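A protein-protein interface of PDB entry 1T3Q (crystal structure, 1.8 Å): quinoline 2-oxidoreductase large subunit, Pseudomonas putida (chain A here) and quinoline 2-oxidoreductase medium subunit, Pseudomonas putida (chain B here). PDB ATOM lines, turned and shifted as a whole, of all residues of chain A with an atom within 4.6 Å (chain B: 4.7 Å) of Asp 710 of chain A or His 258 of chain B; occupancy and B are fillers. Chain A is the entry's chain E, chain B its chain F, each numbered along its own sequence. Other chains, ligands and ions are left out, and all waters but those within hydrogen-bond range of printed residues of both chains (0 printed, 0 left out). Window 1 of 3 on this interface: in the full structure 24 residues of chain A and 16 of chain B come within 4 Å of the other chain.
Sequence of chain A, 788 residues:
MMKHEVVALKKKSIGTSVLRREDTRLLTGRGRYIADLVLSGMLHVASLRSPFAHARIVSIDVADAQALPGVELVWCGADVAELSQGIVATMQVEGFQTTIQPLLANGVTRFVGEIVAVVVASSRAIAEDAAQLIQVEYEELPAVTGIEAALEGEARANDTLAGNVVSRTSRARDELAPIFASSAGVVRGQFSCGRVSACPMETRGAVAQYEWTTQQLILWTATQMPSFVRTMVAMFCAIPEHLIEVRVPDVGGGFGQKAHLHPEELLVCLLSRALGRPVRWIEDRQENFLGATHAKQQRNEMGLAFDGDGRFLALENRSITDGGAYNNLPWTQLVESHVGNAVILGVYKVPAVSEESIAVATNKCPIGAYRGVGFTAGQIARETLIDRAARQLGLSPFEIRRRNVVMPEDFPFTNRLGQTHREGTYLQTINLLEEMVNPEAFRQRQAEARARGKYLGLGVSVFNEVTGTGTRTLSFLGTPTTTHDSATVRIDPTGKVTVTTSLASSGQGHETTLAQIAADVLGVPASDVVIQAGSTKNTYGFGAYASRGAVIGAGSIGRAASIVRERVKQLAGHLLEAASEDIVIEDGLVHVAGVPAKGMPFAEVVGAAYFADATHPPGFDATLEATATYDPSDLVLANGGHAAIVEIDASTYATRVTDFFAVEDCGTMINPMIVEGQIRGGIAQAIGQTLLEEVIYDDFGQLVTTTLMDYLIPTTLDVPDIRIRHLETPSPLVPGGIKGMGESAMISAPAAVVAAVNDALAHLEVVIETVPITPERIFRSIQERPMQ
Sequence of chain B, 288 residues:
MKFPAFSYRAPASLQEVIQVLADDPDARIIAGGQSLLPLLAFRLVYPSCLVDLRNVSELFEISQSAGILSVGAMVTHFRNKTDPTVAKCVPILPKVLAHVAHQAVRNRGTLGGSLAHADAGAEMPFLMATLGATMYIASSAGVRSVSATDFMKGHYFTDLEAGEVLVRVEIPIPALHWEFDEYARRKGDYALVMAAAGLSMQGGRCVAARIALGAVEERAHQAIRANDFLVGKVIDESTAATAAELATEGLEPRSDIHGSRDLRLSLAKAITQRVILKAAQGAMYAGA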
ATOM      1  N   VAL A 704       4.748  30.248 -27.185  1.00  0.00           N
ATOM      2  CA  VAL A 704       3.707  31.013 -26.521  1.00  0.00           C
ATOM      3  C   VAL A 704       3.693  30.846 -25.003  1.00  0.00           C
ATOM      4  O   VAL A 704       2.899  31.477 -24.311  1.00  0.00           O
ATOM      5  CB  VAL A 704       2.320  30.660 -27.101  1.00  0.00           C
ATOM      6  CG1 VAL A 704       2.318  30.921 -28.605  1.00  0.00           C
ATOM      7  CG2 VAL A 704       1.981  29.205 -26.818  1.00  0.00           C
ATOM      8  N   THR A 705       4.576  29.998 -24.485  1.00  0.00           N
ATOM      9  CA  THR A 705       4.658  29.797 -23.041  1.00  0.00           C
ATOM     10  C   THR A 705       6.057  30.179 -22.564  1.00  0.00           C
ATOM     11  O   THR A 705       7.012  29.413 -22.738  1.00  0.00           O
ATOM     12  CB  THR A 705       4.379  28.333 -22.649  1.00  0.00           C
ATOM     13  OG1 THR A 705       5.329  27.474 -23.292  1.00  0.00           O
ATOM     14  CG2 THR A 705       2.974  27.933 -23.067  1.00  0.00           C
ATOM     15  N   THR A 707       6.322  32.223 -19.369  1.00  0.00           N
ATOM     16  CA  THR A 707       6.192  32.737 -18.011  1.00  0.00           C
ATOM     17  C   THR A 707       5.494  31.717 -17.125  1.00  0.00           C
ATOM     18  O   THR A 707       4.848  30.797 -17.613  1.00  0.00           O
ATOM     19  CB  THR A 707       5.367  34.036 -17.976  1.00  0.00           C
ATOM     20  OG1 THR A 707       3.985  33.725 -18.187  1.00  0.00           O
ATOM     21  CG2 THR A 707       5.829  34.992 -19.073  1.00  0.00           C
ATOM     22  N   LEU A 708       5.627  31.893 -15.816  1.00  0.00           N
ATOM     23  CA  LEU A 708       5.002  31.003 -14.850  1.00  0.00           C
ATOM     24  C   LEU A 708       3.489  31.205 -14.806  1.00  0.00           C
ATOM     25  O   LEU A 708       2.780  30.501 -14.089  1.00  0.00           O
ATOM     26  CB  LEU A 708       5.617  31.232 -13.468  1.00  0.00           C
ATOM     27  CG  LEU A 708       6.613  30.177 -12.972  1.00  0.00           C
ATOM     28  CD1 LEU A 708       7.377  29.548 -14.127  1.00  0.00           C
ATOM     29  CD2 LEU A 708       7.557  30.823 -11.971  1.00  0.00           C
ATOM     30  N   MET A 709       2.996  32.177 -15.568  1.00  0.00           N
ATOM     31  CA  MET A 709       1.563  32.418 -15.633  1.00  0.00           C
ATOM     32  C   MET A 709       0.985  31.453 -16.664  1.00  0.00           C
ATOM     33  O   MET A 709      -0.145  30.989 -16.532  1.00  0.00           O
ATOM     34  CB  MET A 709       1.272  33.866 -16.047  1.00  0.00           C
ATOM     35  CG  MET A 709       1.574  34.892 -14.959  1.00  0.00           C
ATOM     36  SD  MET A 709       0.470  34.727 -13.528  1.00  0.00           S
ATOM     37  N   ASP A 710       1.770  31.149 -17.694  1.00  0.00           N
ATOM     38  CA  ASP A 710       1.319  30.231 -18.731  1.00  0.00           C
ATOM     39  C   ASP A 710       1.878  28.822 -18.578  1.00  0.00           C
ATOM     40  O   ASP A 710       1.345  27.881 -19.164  1.00  0.00           O
ATOM     41  CB  ASP A 710       1.660  30.776 -20.116  1.00  0.00           C
ATOM     42  CG  ASP A 710       0.834  31.993 -20.468  1.00  0.00           C
ATOM     43  OD1 ASP A 710      -0.398  31.951 -20.246  1.00  0.00           O
ATOM     44  OD2 ASP A 710       1.405  32.981 -20.967  1.00  0.00           O
ATOM     45  N   TYR A 711       2.955  28.681 -17.814  1.00  0.00           N
ATOM     46  CA  TYR A 711       3.537  27.364 -17.574  1.00  0.00           C
ATOM     47  C   TYR A 711       3.249  27.067 -16.113  1.00  0.00           C
ATOM     48  O   TYR A 711       3.846  27.658 -15.210  1.00  0.00           O
ATOM     49  CB  TYR A 711       5.040  27.357 -17.815  1.00  0.00           C
ATOM     50  CG  TYR A 711       5.608  25.955 -17.845  1.00  0.00           C
ATOM     51  CD1 TYR A 711       5.439  25.139 -18.965  1.00  0.00           C
ATOM     52  CD2 TYR A 711       6.266  25.427 -16.734  1.00  0.00           C
ATOM     53  CE1 TYR A 711       5.912  23.822 -18.978  1.00  0.00           C
ATOM     54  CE2 TYR A 711       6.738  24.121 -16.733  1.00  0.00           C
ATOM     55  CZ  TYR A 711       6.560  23.323 -17.854  1.00  0.00           C
ATOM     56  OH  TYR A 711       7.025  22.025 -17.843  1.00  0.00           O
ATOM     57  N   LEU A 712       2.331  26.136 -15.892  1.00  0.00           N
ATOM     58  CA  LEU A 712       1.891  25.793 -14.554  1.00  0.00           C
ATOM     59  C   LEU A 712       2.554  24.587 -13.919  1.00  0.00           C
ATOM     60  O   LEU A 712       2.400  23.465 -14.402  1.00  0.00           O
ATOM     61  CB  LEU A 712       0.380  25.573 -14.589  1.00  0.00           C
ATOM     62  CG  LEU A 712      -0.343  26.604 -15.461  1.00  0.00           C
ATOM     63  CD1 LEU A 712      -1.799  26.208 -15.643  1.00  0.00           C
ATOM     64  CD2 LEU A 712      -0.210  27.980 -14.821  1.00  0.00           C
ATOM     65  N   LEU B 192     -11.044  31.477 -15.456  1.00  0.00           N
ATOM     66  CA  LEU B 192     -11.415  31.311 -16.857  1.00  0.00           C
ATOM     67  C   LEU B 192     -12.799  31.936 -16.998  1.00  0.00           C
ATOM     68  O   LEU B 192     -13.153  32.477 -18.044  1.00  0.00           O
ATOM     69  CB  LEU B 192     -11.475  29.827 -17.233  1.00  0.00           C
ATOM     70  CG  LEU B 192     -10.168  29.029 -17.177  1.00  0.00           C
ATOM     71  CD1 LEU B 192     -10.420  27.600 -17.621  1.00  0.00           C
ATOM     72  CD2 LEU B 192      -9.134  29.683 -18.073  1.00  0.00           C
ATOM     73  N   ASP B 256      -7.814  30.025 -26.235  1.00  0.00           N
ATOM     74  CA  ASP B 256      -6.384  30.207 -26.031  1.00  0.00           C
ATOM     75  C   ASP B 256      -5.831  28.910 -25.459  1.00  0.00           C
ATOM     76  O   ASP B 256      -6.548  27.912 -25.377  1.00  0.00           O
ATOM     77  CB  ASP B 256      -6.079  31.392 -25.103  1.00  0.00           C
ATOM     78  CG  ASP B 256      -6.713  31.256 -23.736  1.00  0.00           C
ATOM     79  OD1 ASP B 256      -6.771  30.132 -23.196  1.00  0.00           O
ATOM     80  OD2 ASP B 256      -7.138  32.296 -23.192  1.00  0.00           O
ATOM     81  N   ILE B 257      -4.567  28.915 -25.058  1.00  0.00           N
ATOM     82  CA  ILE B 257      -3.955  27.700 -24.544  1.00  0.00           C
ATOM     83  C   ILE B 257      -4.568  27.165 -23.254  1.00  0.00           C
ATOM     84  O   ILE B 257      -4.366  26.003 -22.901  1.00  0.00           O
ATOM     85  CB  ILE B 257      -2.435  27.895 -24.342  1.00  0.00           C
ATOM     86  CG1 ILE B 257      -2.170  28.931 -23.251  1.00  0.00           C
ATOM     87  CG2 ILE B 257      -1.802  28.357 -25.648  1.00  0.00           C
ATOM     88  CD1 ILE B 257      -0.717  28.990 -22.815  1.00  0.00           C
ATOM     89  N   HIS B 258      -5.334  27.995 -22.553  1.00  0.00           N
ATOM     90  CA  HIS B 258      -5.938  27.548 -21.306  1.00  0.00           C
ATOM     91  C   HIS B 258      -7.390  27.112 -21.444  1.00  0.00           C
ATOM     92  O   HIS B 258      -8.033  26.765 -20.459  1.00  0.00           O
ATOM     93  CB  HIS B 258      -5.813  28.640 -20.242  1.00  0.00           C
ATOM     94  CG  HIS B 258      -4.399  28.928 -19.846  1.00  0.00           C
ATOM     95  ND1 HIS B 258      -3.787  30.139 -20.089  1.00  0.00           N
ATOM     96  CD2 HIS B 258      -3.462  28.144 -19.259  1.00  0.00           C
ATOM     97  CE1 HIS B 258      -2.534  30.088 -19.672  1.00  0.00           C
ATOM     98  NE2 HIS B 258      -2.311  28.889 -19.164  1.00  0.00           N
ATOM     99  N   GLY B 259      -7.904  27.120 -22.667  1.00  0.00           N
ATOM    100  CA  GLY B 259      -9.279  26.703 -22.867  1.00  0.00           C
ATOM    101  C   GLY B 259      -9.915  27.218 -24.141  1.00  0.00           C
ATOM    102  O   GLY B 259      -9.734  28.381 -24.514  1.00  0.00           O
ATOM    103  N   LEU B 263     -15.224  25.123 -24.164  1.00  0.00           N
ATOM    104  CA  LEU B 263     -14.937  24.789 -22.776  1.00  0.00           C
ATOM    105  C   LEU B 263     -15.379  25.940 -21.880  1.00  0.00           C
ATOM    106  O   LEU B 263     -16.012  25.725 -20.845  1.00  0.00           O
ATOM    107  CB  LEU B 263     -13.440  24.539 -22.577  1.00  0.00           C
ATOM    108  CG  LEU B 263     -13.009  24.373 -21.117  1.00  0.00           C
ATOM    109  CD1 LEU B 263     -13.686  23.158 -20.508  1.00  0.00           C
ATOM    110  CD2 LEU B 263     -11.497  24.243 -21.049  1.00  0.00           C
ATOM    111  N   ARG B 264     -15.036  27.157 -22.298  1.00  0.00           N
ATOM    112  CA  ARG B 264     -15.368  28.387 -21.578  1.00  0.00           C
ATOM    113  C   ARG B 264     -16.868  28.501 -21.339  1.00  0.00           C
ATOM    114  O   ARG B 264     -17.317  28.798 -20.229  1.00  0.00           O
ATOM    115  CB  ARG B 264     -14.921  29.602 -22.388  1.00  0.00           C
ATOM    116  CG  ARG B 264     -13.477  29.570 -22.831  1.00  0.00           C
ATOM    117  CD  ARG B 264     -12.600  30.204 -21.808  1.00  0.00           C
ATOM    118  NE  ARG B 264     -11.205  30.290 -22.222  1.00  0.00           N
ATOM    119  CZ  ARG B 264     -10.292  30.959 -21.531  1.00  0.00           C
ATOM    120  NH1 ARG B 264     -10.649  31.587 -20.423  1.00  0.00           N
ATOM    121  NH2 ARG B 264      -9.028  30.981 -21.922  1.00  0.00           N
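OD1 of Asp 256 of chain B lies within hydrogen-bond range of N of His 258 of chain B (2.7 Å).
OG1 of Thr 707 of chain A sits at hydrogen-bond distance from N of Asp 710 of chain A.
Among the printed residues, pairs that only touch across the chains: Thr 705 of chain A with Ile 257 of chain B (3.8 Å), Asp 710 of chain A with Ile 257 of chain B (3.9 Å) and Asp 710 of chain A with His 258 of chain B (2.9 Å).
Asp 710 of chain A touches just these residues of chain B: Ile 257 and His 258.
Of the printed residues of chain A, His 258 of chain B touches Asp 710 (2.9 Å).
Printed residues of chain B within 4 Å of Thr 705 of chain A: Ile 257.
Of the printed residues of chain A, Ile 257 of chain B touches Thr 705 and Asp 710.
Tyr 711 of chain A touches none of the printed residues of chain B.
The nearest printed residue of chain B that does not touch Asp 710 of chain A is Asp 256 of chain B (7.2 Å).
The nearest printed residue of chain A that does not touch His 258 of chain B is Met 709 of chain A (4.004 Å).
The nearest printed residue of chain A that does not touch Ile 257 of chain B is Val 704 of chain A (4.05 Å).
Along chain B the printed residues that touch a printed residue of chain A span positions 257 to 258.
Printed residues of chain A that touch a printed residue of chain B: Thr 705 and Asp 710.
Among the printed residues, 3 pairs touch across the chains.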
